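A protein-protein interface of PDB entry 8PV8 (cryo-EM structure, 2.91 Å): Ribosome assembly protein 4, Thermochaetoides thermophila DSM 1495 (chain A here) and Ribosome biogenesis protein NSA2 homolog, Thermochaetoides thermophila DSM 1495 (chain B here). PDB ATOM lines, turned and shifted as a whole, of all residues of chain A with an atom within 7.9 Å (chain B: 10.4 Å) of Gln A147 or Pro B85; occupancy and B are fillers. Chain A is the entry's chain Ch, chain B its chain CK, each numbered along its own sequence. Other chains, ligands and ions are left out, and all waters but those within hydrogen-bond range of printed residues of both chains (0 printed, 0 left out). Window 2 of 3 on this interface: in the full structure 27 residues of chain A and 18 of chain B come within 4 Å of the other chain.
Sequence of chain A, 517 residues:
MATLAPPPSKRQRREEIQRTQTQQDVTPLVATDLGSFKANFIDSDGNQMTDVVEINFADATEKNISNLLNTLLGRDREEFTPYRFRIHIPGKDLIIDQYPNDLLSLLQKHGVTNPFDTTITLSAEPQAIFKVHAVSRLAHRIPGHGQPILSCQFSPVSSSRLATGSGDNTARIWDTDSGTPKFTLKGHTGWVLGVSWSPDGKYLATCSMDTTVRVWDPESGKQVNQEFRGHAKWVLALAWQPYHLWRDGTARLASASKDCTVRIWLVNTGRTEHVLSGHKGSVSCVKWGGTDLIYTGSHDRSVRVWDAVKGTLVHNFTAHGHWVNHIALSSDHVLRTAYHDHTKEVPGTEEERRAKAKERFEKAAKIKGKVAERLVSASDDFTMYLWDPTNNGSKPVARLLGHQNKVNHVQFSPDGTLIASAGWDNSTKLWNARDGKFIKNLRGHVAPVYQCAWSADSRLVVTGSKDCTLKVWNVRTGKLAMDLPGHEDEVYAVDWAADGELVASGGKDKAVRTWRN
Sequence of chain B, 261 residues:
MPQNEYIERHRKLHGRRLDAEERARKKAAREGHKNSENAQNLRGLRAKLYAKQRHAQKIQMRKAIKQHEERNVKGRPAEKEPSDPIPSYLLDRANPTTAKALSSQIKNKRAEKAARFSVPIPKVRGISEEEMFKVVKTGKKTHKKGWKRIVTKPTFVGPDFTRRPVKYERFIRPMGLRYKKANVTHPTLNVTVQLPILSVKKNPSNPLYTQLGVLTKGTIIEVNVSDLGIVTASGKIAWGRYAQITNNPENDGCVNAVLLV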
ATOM      1  N   GLY A 144      19.981  16.832  27.706  1.00  0.00           N
ATOM      2  CA  GLY A 144      20.950  16.313  26.762  1.00  0.00           C
ATOM      3  C   GLY A 144      20.324  15.732  25.513  1.00  0.00           C
ATOM      4  O   GLY A 144      20.924  15.772  24.435  1.00  0.00           O
ATOM      5  N   HIS A 145      19.121  15.186  25.644  1.00  0.00           N
ATOM      6  CA  HIS A 145      18.391  14.704  24.485  1.00  0.00           C
ATOM      7  C   HIS A 145      17.626  15.847  23.833  1.00  0.00           C
ATOM      8  O   HIS A 145      16.895  16.592  24.493  1.00  0.00           O
ATOM      9  CB  HIS A 145      17.419  13.591  24.877  1.00  0.00           C
ATOM     10  CG  HIS A 145      18.072  12.261  25.098  1.00  0.00           C
ATOM     11  ND1 HIS A 145      18.612  11.518  24.070  1.00  0.00           N
ATOM     12  CD2 HIS A 145      18.255  11.533  26.225  1.00  0.00           C
ATOM     13  CE1 HIS A 145      19.100  10.390  24.553  1.00  0.00           C
ATOM     14  NE2 HIS A 145      18.901  10.377  25.859  1.00  0.00           N
ATOM     15  N   GLY A 146      17.805  15.988  22.523  1.00  0.00           N
ATOM     16  CA  GLY A 146      17.102  16.989  21.755  1.00  0.00           C
ATOM     17  C   GLY A 146      15.728  16.575  21.290  1.00  0.00           C
ATOM     18  O   GLY A 146      15.029  17.381  20.667  1.00  0.00           O
ATOM     19  N   GLN A 147      15.320  15.340  21.567  1.00  0.00           N
ATOM     20  CA  GLN A 147      14.030  14.789  21.174  1.00  0.00           C
ATOM     21  C   GLN A 147      13.459  14.010  22.356  1.00  0.00           C
ATOM     22  O   GLN A 147      14.200  13.724  23.305  1.00  0.00           O
ATOM     23  CB  GLN A 147      14.186  13.908  19.929  1.00  0.00           C
ATOM     24  CG  GLN A 147      14.593  14.659  18.669  1.00  0.00           C
ATOM     25  CD  GLN A 147      13.496  15.566  18.150  1.00  0.00           C
ATOM     26  OE1 GLN A 147      12.311  15.293  18.328  1.00  0.00           O
ATOM     27  NE2 GLN A 147      13.889  16.658  17.505  1.00  0.00           N
ATOM     28  N   PRO A 148      12.154  13.702  22.371  1.00  0.00           N
ATOM     29  CA  PRO A 148      11.587  12.931  23.488  1.00  0.00           C
ATOM     30  C   PRO A 148      12.233  11.563  23.667  1.00  0.00           C
ATOM     31  O   PRO A 148      12.548  10.868  22.699  1.00  0.00           O
ATOM     32  CB  PRO A 148      10.113  12.796  23.102  1.00  0.00           C
ATOM     33  CG  PRO A 148       9.837  14.007  22.311  1.00  0.00           C
ATOM     34  CD  PRO A 148      11.088  14.287  21.532  1.00  0.00           C
ATOM     35  N   ILE A 149      12.425  11.187  24.931  1.00  0.00           N
ATOM     36  CA  ILE A 149      13.026   9.902  25.266  1.00  0.00           C
ATOM     37  C   ILE A 149      11.997   8.798  25.067  1.00  0.00           C
ATOM     38  O   ILE A 149      10.858   8.897  25.540  1.00  0.00           O
ATOM     39  CB  ILE A 149      13.556   9.920  26.707  1.00  0.00           C
ATOM     40  CG1 ILE A 149      14.592  11.031  26.880  1.00  0.00           C
ATOM     41  CG2 ILE A 149      14.151   8.572  27.087  1.00  0.00           C
ATOM     42  CD1 ILE A 149      15.044  11.225  28.307  1.00  0.00           C
ATOM     43  N   LEU A 150      12.394   7.738  24.364  1.00  0.00           N
ATOM     44  CA  LEU A 150      11.486   6.645  24.053  1.00  0.00           C
ATOM     45  C   LEU A 150      11.714   5.390  24.884  1.00  0.00           C
ATOM     46  O   LEU A 150      10.764   4.623  25.076  1.00  0.00           O
ATOM     47  CB  LEU A 150      11.576   6.289  22.563  1.00  0.00           C
ATOM     48  CG  LEU A 150      11.463   7.475  21.607  1.00  0.00           C
ATOM     49  CD1 LEU A 150      11.633   7.024  20.166  1.00  0.00           C
ATOM     50  CD2 LEU A 150      10.136   8.188  21.797  1.00  0.00           C
ATOM     51  N   GLY A 165      17.308   5.608  25.192  1.00  0.00           N
ATOM     52  CA  GLY A 165      17.297   5.744  23.744  1.00  0.00           C
ATOM     53  C   GLY A 165      16.171   6.659  23.326  1.00  0.00           C
ATOM     54  O   GLY A 165      15.034   6.509  23.782  1.00  0.00           O
ATOM     55  N   SER A 166      16.493   7.618  22.454  1.00  0.00           N
ATOM     56  CA  SER A 166      15.544   8.682  22.155  1.00  0.00           C
ATOM     57  C   SER A 166      15.332   8.819  20.655  1.00  0.00           C
ATOM     58  O   SER A 166      15.874   8.061  19.849  1.00  0.00           O
ATOM     59  CB  SER A 166      16.006  10.022  22.735  1.00  0.00           C
ATOM     60  OG  SER A 166      15.056  11.041  22.481  1.00  0.00           O
ATOM     61  N   GLY A 167      14.516   9.810  20.297  1.00  0.00           N
ATOM     62  CA  GLY A 167      14.198  10.155  18.929  1.00  0.00           C
ATOM     63  C   GLY A 167      15.185  11.069  18.249  1.00  0.00           C
ATOM     64  O   GLY A 167      14.968  11.462  17.101  1.00  0.00           O
ATOM     65  N   ASP A 168      16.268  11.435  18.929  1.00  0.00           N
ATOM     66  CA  ASP A 168      17.342  12.210  18.326  1.00  0.00           C
ATOM     67  C   ASP A 168      18.390  11.326  17.667  1.00  0.00           C
ATOM     68  O   ASP A 168      19.559  11.722  17.599  1.00  0.00           O
ATOM     69  CB  ASP A 168      17.990  13.128  19.368  1.00  0.00           C
ATOM     70  CG  ASP A 168      18.490  12.378  20.594  1.00  0.00           C
ATOM     71  OD1 ASP A 168      18.333  11.141  20.668  1.00  0.00           O
ATOM     72  OD2 ASP A 168      19.053  13.036  21.493  1.00  0.00           O
ATOM     73  N   ASN A 169      17.993  10.125  17.236  1.00  0.00           N
ATOM     74  CA  ASN A 169      18.821   9.136  16.552  1.00  0.00           C
ATOM     75  C   ASN A 169      19.953   8.609  17.424  1.00  0.00           C
ATOM     76  O   ASN A 169      20.906   8.017  16.908  1.00  0.00           O
ATOM     77  CB  ASN A 169      19.383   9.688  15.235  1.00  0.00           C
ATOM     78  CG  ASN A 169      18.309   9.890  14.185  1.00  0.00           C
ATOM     79  OD1 ASN A 169      17.117   9.885  14.489  1.00  0.00           O
ATOM     80  ND2 ASN A 169      18.730  10.093  12.943  1.00  0.00           N
ATOM     81  N   THR A 170      19.877   8.804  18.741  1.00  0.00           N
ATOM     82  CA  THR A 170      20.968   8.443  19.632  1.00  0.00           C
ATOM     83  C   THR A 170      20.449   7.711  20.862  1.00  0.00           C
ATOM     84  O   THR A 170      19.265   7.783  21.225  1.00  0.00           O
ATOM     85  CB  THR A 170      21.783   9.663  20.112  1.00  0.00           C
ATOM     86  OG1 THR A 170      20.956  10.508  20.921  1.00  0.00           O
ATOM     87  CG2 THR A 170      22.370  10.462  18.950  1.00  0.00           C
ATOM     88  N   TRP A 191      14.888   6.960  14.996  1.00  0.00           N
ATOM     89  CA  TRP A 191      14.654   7.002  16.436  1.00  0.00           C
ATOM     90  C   TRP A 191      15.000   5.664  17.070  1.00  0.00           C
ATOM     91  O   TRP A 191      14.569   4.609  16.601  1.00  0.00           O
ATOM     92  CB  TRP A 191      13.193   7.332  16.751  1.00  0.00           C
ATOM     93  CG  TRP A 191      12.587   8.462  15.991  1.00  0.00           C
ATOM     94  CD1 TRP A 191      13.224   9.544  15.462  1.00  0.00           C
ATOM     95  CD2 TRP A 191      11.203   8.615  15.670  1.00  0.00           C
ATOM     96  NE1 TRP A 191      12.320  10.366  14.837  1.00  0.00           N
ATOM     97  CE2 TRP A 191      11.071   9.815  14.951  1.00  0.00           C
ATOM     98  CE3 TRP A 191      10.060   7.852  15.926  1.00  0.00           C
ATOM     99  CZ2 TRP A 191       9.844  10.270  14.483  1.00  0.00           C
ATOM    100  CZ3 TRP A 191       8.844   8.304  15.460  1.00  0.00           C
ATOM    101  CH2 TRP A 191       8.745   9.502  14.745  1.00  0.00           C
ATOM    102  N   VAL A 192      15.764   5.711  18.156  1.00  0.00           N
ATOM    103  CA  VAL A 192      16.133   4.511  18.898  1.00  0.00           C
ATOM    104  C   VAL A 192      14.922   4.090  19.723  1.00  0.00           C
ATOM    105  O   VAL A 192      14.663   4.646  20.793  1.00  0.00           O
ATOM    106  CB  VAL A 192      17.359   4.752  19.784  1.00  0.00           C
ATOM    107  CG1 VAL A 192      17.717   3.489  20.548  1.00  0.00           C
ATOM    108  CG2 VAL A 192      18.529   5.203  18.937  1.00  0.00           C
ATOM    109  N   LEU A 193      14.169   3.116  19.219  1.00  0.00           N
ATOM    110  CA  LEU A 193      12.963   2.674  19.901  1.00  0.00           C
ATOM    111  C   LEU A 193      13.236   1.771  21.091  1.00  0.00           C
ATOM    112  O   LEU A 193      12.393   1.695  21.991  1.00  0.00           O
ATOM    113  CB  LEU A 193      12.035   1.931  18.942  1.00  0.00           C
ATOM    114  CG  LEU A 193      11.566   2.609  17.666  1.00  0.00           C
ATOM    115  CD1 LEU A 193      10.921   1.546  16.815  1.00  0.00           C
ATOM    116  CD2 LEU A 193      10.581   3.719  17.978  1.00  0.00           C
ATOM    117  N   MET A 209      14.397   2.844  14.303  1.00  0.00           N
ATOM    118  CA  MET A 209      13.510   3.044  13.157  1.00  0.00           C
ATOM    119  C   MET A 209      14.145   2.676  11.827  1.00  0.00           C
ATOM    120  O   MET A 209      13.416   2.381  10.874  1.00  0.00           O
ATOM    121  CB  MET A 209      13.073   4.510  13.077  1.00  0.00           C
ATOM    122  CG  MET A 209      12.209   4.993  14.211  1.00  0.00           C
ATOM    123  SD  MET A 209      10.656   4.109  14.342  1.00  0.00           S
ATOM    124  CE  MET A 209       9.834   4.699  12.871  1.00  0.00           C
ATOM    125  N   TYR A 492       6.959   8.629  28.927  1.00  0.00           N
ATOM    126  CA  TYR A 492       7.000   7.511  27.994  1.00  0.00           C
ATOM    127  C   TYR A 492       7.677   6.267  28.543  1.00  0.00           C
ATOM    128  O   TYR A 492       7.184   5.162  28.306  1.00  0.00           O
ATOM    129  CB  TYR A 492       7.713   7.926  26.702  1.00  0.00           C
ATOM    130  CG  TYR A 492       6.899   8.836  25.815  1.00  0.00           C
ATOM    131  CD1 TYR A 492       5.521   8.694  25.720  1.00  0.00           C
ATOM    132  CD2 TYR A 492       7.507   9.838  25.073  1.00  0.00           C
ATOM    133  CE1 TYR A 492       4.771   9.524  24.910  1.00  0.00           C
ATOM    134  CE2 TYR A 492       6.766  10.674  24.261  1.00  0.00           C
ATOM    135  CZ  TYR A 492       5.400  10.513  24.183  1.00  0.00           C
ATOM    136  OH  TYR A 492       4.660  11.343  23.374  1.00  0.00           O
ATOM    137  N   GLY A 507      10.416  11.132  29.069  1.00  0.00           N
ATOM    138  CA  GLY A 507       9.234  11.347  28.261  1.00  0.00           C
ATOM    139  C   GLY A 507       9.372  12.424  27.210  1.00  0.00           C
ATOM    140  O   GLY A 507      10.434  12.582  26.601  1.00  0.00           O
ATOM    141  N   LYS A 508       8.295  13.177  26.993  1.00  0.00           N
ATOM    142  CA  LYS A 508       8.272  14.189  25.946  1.00  0.00           C
ATOM    143  C   LYS A 508       8.934  15.493  26.373  1.00  0.00           C
ATOM    144  O   LYS A 508       9.085  16.395  25.544  1.00  0.00           O
ATOM    145  CB  LYS A 508       6.829  14.444  25.509  1.00  0.00           C
ATOM    146  CG  LYS A 508       6.659  14.802  24.042  1.00  0.00           C
ATOM    147  CD  LYS A 508       5.190  14.846  23.655  1.00  0.00           C
ATOM    148  CE  LYS A 508       5.005  15.385  22.247  1.00  0.00           C
ATOM    149  NZ  LYS A 508       3.567  15.551  21.902  1.00  0.00           N
ATOM    150  N   ASP A 509       9.341  15.610  27.640  1.00  0.00           N
ATOM    151  CA  ASP A 509      10.030  16.808  28.106  1.00  0.00           C
ATOM    152  C   ASP A 509      11.507  16.828  27.732  1.00  0.00           C
ATOM    153  O   ASP A 509      12.183  17.821  28.021  1.00  0.00           O
ATOM    154  CB  ASP A 509       9.873  16.948  29.621  1.00  0.00           C
ATOM    155  CG  ASP A 509      10.274  15.691  30.372  1.00  0.00           C
ATOM    156  OD1 ASP A 509      10.612  14.679  29.721  1.00  0.00           O
ATOM    157  OD2 ASP A 509      10.251  15.715  31.620  1.00  0.00           O
ATOM    158  N   LYS A 510      12.019  15.748  27.136  1.00  0.00           N
ATOM    159  CA  LYS A 510      13.354  15.557  26.575  1.00  0.00           C
ATOM    160  C   LYS A 510      14.449  15.494  27.642  1.00  0.00           C
ATOM    161  O   LYS A 510      15.621  15.377  27.284  1.00  0.00           O
ATOM    162  CB  LYS A 510      13.737  16.628  25.533  1.00  0.00           C
ATOM    163  CG  LYS A 510      12.707  16.815  24.428  1.00  0.00           C
ATOM    164  CD  LYS A 510      13.167  17.833  23.396  1.00  0.00           C
ATOM    165  CE  LYS A 510      13.562  19.149  24.044  1.00  0.00           C
ATOM    166  NZ  LYS A 510      12.431  19.756  24.796  1.00  0.00           N
ATOM    167  N   ALA A 511      14.120  15.561  28.928  1.00  0.00           N
ATOM    168  CA  ALA A 511      15.108  15.479  29.994  1.00  0.00           C
ATOM    169  C   ALA A 511      14.830  14.267  30.871  1.00  0.00           C
ATOM    170  O   ALA A 511      13.693  14.044  31.297  1.00  0.00           O
ATOM    171  CB  ALA A 511      15.104  16.751  30.843  1.00  0.00           C
ATOM    172  N   GLU B  81       7.530   7.649   8.214  1.00  0.00           N
ATOM    173  CA  GLU B  81       7.947   7.990   9.567  1.00  0.00           C
ATOM    174  C   GLU B  81       7.214   9.237  10.062  1.00  0.00           C
ATOM    175  O   GLU B  81       7.183  10.252   9.364  1.00  0.00           O
ATOM    176  CB  GLU B  81       9.461   8.203   9.622  1.00  0.00           C
ATOM    177  CG  GLU B  81       9.977   8.695  10.963  1.00  0.00           C
ATOM    178  CD  GLU B  81      11.477   8.536  11.102  1.00  0.00           C
ATOM    179  OE1 GLU B  81      12.079   7.823  10.271  1.00  0.00           O
ATOM    180  OE2 GLU B  81      12.055   9.123  12.039  1.00  0.00           O
ATOM    181  N   PRO B  82       6.609   9.145  11.249  1.00  0.00           N
ATOM    182  CA  PRO B  82       5.904  10.301  11.819  1.00  0.00           C
ATOM    183  C   PRO B  82       6.835  11.475  12.089  1.00  0.00           C
ATOM    184  O   PRO B  82       8.060  11.345  12.128  1.00  0.00           O
ATOM    185  CB  PRO B  82       5.322   9.759  13.134  1.00  0.00           C
ATOM    186  CG  PRO B  82       5.596   8.286  13.153  1.00  0.00           C
ATOM    187  CD  PRO B  82       6.156   7.875  11.838  1.00  0.00           C
ATOM    188  N   SER B  83       6.226  12.650  12.261  1.00  0.00           N
ATOM    189  CA  SER B  83       7.002  13.856  12.534  1.00  0.00           C
ATOM    190  C   SER B  83       7.506  13.880  13.973  1.00  0.00           C
ATOM    191  O   SER B  83       8.650  14.270  14.233  1.00  0.00           O
ATOM    192  CB  SER B  83       6.161  15.098  12.239  1.00  0.00           C
ATOM    193  OG  SER B  83       6.853  16.278  12.604  1.00  0.00           O
ATOM    194  N   ASP B  84       6.667  13.465  14.924  1.00  0.00           N
ATOM    195  CA  ASP B  84       7.002  13.565  16.338  1.00  0.00           C
ATOM    196  C   ASP B  84       7.414  12.204  16.873  1.00  0.00           C
ATOM    197  O   ASP B  84       6.737  11.206  16.577  1.00  0.00           O
ATOM    198  CB  ASP B  84       5.816  14.102  17.130  1.00  0.00           C
ATOM    199  CG  ASP B  84       6.171  14.412  18.569  1.00  0.00           C
ATOM    200  OD1 ASP B  84       6.841  15.438  18.810  1.00  0.00           O
ATOM    201  OD2 ASP B  84       5.782  13.630  19.460  1.00  0.00           O
ATOM    202  N   PRO B  85       8.503  12.110  17.648  1.00  0.00           N
ATOM    203  CA  PRO B  85       8.923  10.809  18.191  1.00  0.00           C
ATOM    204  C   PRO B  85       7.948  10.233  19.205  1.00  0.00           C
ATOM    205  O   PRO B  85       7.568  10.902  20.172  1.00  0.00           O
ATOM    206  CB  PRO B  85      10.274  11.125  18.845  1.00  0.00           C
ATOM    207  CG  PRO B  85      10.756  12.352  18.150  1.00  0.00           C
ATOM    208  CD  PRO B  85       9.521  13.150  17.863  1.00  0.00           C
ATOM    209  N   ILE B  86       7.541   8.990  18.988  1.00  0.00           N
ATOM    210  CA  ILE B  86       6.635   8.280  19.886  1.00  0.00           C
ATOM    211  C   ILE B  86       7.228   6.901  20.135  1.00  0.00           C
ATOM    212  O   ILE B  86       7.972   6.373  19.291  1.00  0.00           O
ATOM    213  CB  ILE B  86       5.202   8.201  19.309  1.00  0.00           C
ATOM    214  CG1 ILE B  86       5.232   7.676  17.874  1.00  0.00           C
ATOM    215  CG2 ILE B  86       4.508   9.554  19.391  1.00  0.00           C
ATOM    216  CD1 ILE B  86       3.864   7.512  17.256  1.00  0.00           C
ATOM    217  N   PRO B  87       6.939   6.290  21.285  1.00  0.00           N
ATOM    218  CA  PRO B  87       7.474   4.950  21.565  1.00  0.00           C
ATOM    219  C   PRO B  87       6.844   3.884  20.678  1.00  0.00           C
ATOM    220  O   PRO B  87       5.952   4.140  19.869  1.00  0.00           O
ATOM    221  CB  PRO B  87       7.134   4.716  23.040  1.00  0.00           C
ATOM    222  CG  PRO B  87       6.816   6.052  23.592  1.00  0.00           C
ATOM    223  CD  PRO B  87       6.283   6.873  22.469  1.00  0.00           C
ATOM    224  N   SER B  88       7.338   2.655  20.853  1.00  0.00           N
ATOM    225  CA  SER B  88       6.928   1.554  19.985  1.00  0.00           C
ATOM    226  C   SER B  88       5.483   1.142  20.226  1.00  0.00           C
ATOM    227  O   SER B  88       4.826   0.630  19.312  1.00  0.00           O
ATOM    228  CB  SER B  88       7.858   0.357  20.185  1.00  0.00           C
ATOM    229  OG  SER B  88       7.791  -0.122  21.515  1.00  0.00           O
ATOM    230  N   TYR B  89       4.967   1.349  21.437  1.00  0.00           N
ATOM    231  CA  TYR B  89       3.586   0.987  21.724  1.00  0.00           C
ATOM    232  C   TYR B  89       2.588   2.042  21.265  1.00  0.00           C
ATOM    233  O   TYR B  89       1.379   1.806  21.355  1.00  0.00           O
ATOM    234  CB  TYR B  89       3.406   0.707  23.221  1.00  0.00           C
ATOM    235  CG  TYR B  89       3.967   1.759  24.157  1.00  0.00           C
ATOM    236  CD1 TYR B  89       3.276   2.939  24.411  1.00  0.00           C
ATOM    237  CD2 TYR B  89       5.179   1.560  24.804  1.00  0.00           C
ATOM    238  CE1 TYR B  89       3.784   3.895  25.269  1.00  0.00           C
ATOM    239  CE2 TYR B  89       5.694   2.510  25.664  1.00  0.00           C
ATOM    240  CZ  TYR B  89       4.992   3.674  25.893  1.00  0.00           C
ATOM    241  OH  TYR B  89       5.502   4.621  26.748  1.00  0.00           O
ATOM    242  N   LEU B  90       3.057   3.190  20.778  1.00  0.00           N
ATOM    243  CA  LEU B  90       2.187   4.219  20.229  1.00  0.00           C
ATOM    244  C   LEU B  90       2.274   4.305  18.711  1.00  0.00           C
ATOM    245  O   LEU B  90       1.621   5.163  18.109  1.00  0.00           O
ATOM    246  CB  LEU B  90       2.514   5.578  20.851  1.00  0.00           C
ATOM    247  CG  LEU B  90       2.114   5.736  22.317  1.00  0.00           C
ATOM    248  CD1 LEU B  90       2.507   7.106  22.839  1.00  0.00           C
ATOM    249  CD2 LEU B  90       0.625   5.504  22.486  1.00  0.00           C
ATOM    250  N   LEU B  91       3.062   3.437  18.081  1.00  0.00           N
ATOM    251  CA  LEU B  91       3.165   3.418  16.632  1.00  0.00           C
ATOM    252  C   LEU B  91       1.912   2.805  16.014  1.00  0.00           C
ATOM    253  O   LEU B  91       1.170   2.059  16.658  1.00  0.00           O
ATOM    254  CB  LEU B  91       4.403   2.641  16.188  1.00  0.00           C
ATOM    255  CG  LEU B  91       5.752   3.252  16.561  1.00  0.00           C
ATOM    256  CD1 LEU B  91       6.882   2.312  16.185  1.00  0.00           C
ATOM    257  CD2 LEU B  91       5.926   4.598  15.881  1.00  0.00           C
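The side-chain amino group of Lys A508 is in salt-bridge range of the side-chain carboxylate of Asp B84, 3.8 Å away.
The side-chain carboxylate (OE2) of Glu B81 is in hydrogen-bond range of the indole nitrogen (NE1) of Trp A191 (3.1 Å).
OH of Tyr B89 sits close to O of Tyr A492 (2.4 Å).
N of Leu A150 sits at hydrogen-bond distance from O of Gly A165 (3.0 Å).
The backbone carbonyl oxygen of Pro A148 is in hydrogen-bond range of the side-chain hydroxyl of Ser A166.
OG of Ser A166 lies within hydrogen-bond range of O of Gln A147.
O of Pro A148 lies within hydrogen-bond range of N of Gly A167 (3.3 Å).
O of Trp A191 sits at hydrogen-bond distance from N of Met A209 (2.9 Å).
Among the printed residues, merely in contact across the chains: Gln A147 with Pro B85 (3.3 Å), Pro A148 with Pro B85 (3.9 Å), Leu A150 with Pro B85 (3.96 Å), Leu A150 with Ile B86 (3.6 Å), Leu A150 with Pro B87 (3.8 Å), Trp A191 with Pro B82 (3.1 Å), Trp A191 with Asp B84 (3.2 Å), Trp A191 with Pro B85 (3.7 Å), Trp A191 with Ile B86 (3.8 Å), Leu A193 with Ile B86 (3.9 Å), Tyr A492 with Pro B87 (3.6 Å) and Tyr A492 with Leu B90 (3.9 Å).
No residue of chain B comes within 4 Å of His A145.
No residue of chain B comes within 4 Å of Gly A146.
Gln A147 touches just one residue of chain B: Pro B85.
Pro A148 touches just one residue of chain B: Pro B85 (3.9 Å).
Of the printed residues of chain B, Leu A150 touches Pro B85 (3.96 Å), Ile B86 (3.6 Å) and Pro B87 (3.8 Å).
No residue of chain B comes within 4 Å of Asp A168.
Of the printed residues of chain B, Trp A191 touches Glu B81 (3.1 Å), Pro B82 (3.1 Å), Asp B84 (3.2 Å), Pro B85 (3.7 Å) and Ile B86 (3.8 Å).
Printed residues of chain B within 4 Å of Lys A508: Asp B84.
Lys A510 touches none of the printed residues of chain B.
Ala A511 touches none of the printed residues of chain B.
Printed residues of chain A within 4 Å of Glu B81: Trp A191 (3.1 Å).
Of chain A, only Gln A147 (3.3 Å), Pro A148 (3.9 Å), Leu A150 (3.96 Å) and Trp A191 (3.7 Å) come within 4 Å of Pro B85.
Of the printed residues of chain A, Tyr B89 touches Tyr A492.
The nearest printed residue of chain B that does not touch Leu A150 is Tyr B89 (5.5 Å).
Of the 11 printed residues of chain B, 8 touch a printed residue of chain A.
Hydrophobic or aromatic side chains of chain B that line the printed part of chain A: Pro B82, Pro B85, Pro B87, Tyr B89 and Leu B90.
Of the 23 printed residues of chain A, 7 touch a printed residue of chain B.
Printed residues of chain A that touch a printed residue of chain B: Gln A147, Pro A148, Leu A150, Trp A191, Leu A193, Tyr A492 and Lys A508.
Among the printed residues, 15 pairs touch across the chains.
Among the printed residues, Asp or Glu carboxylates within 4 Å of a Lys or Arg side-chain nitrogen of the other chain: Lys A508 with Asp B84.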
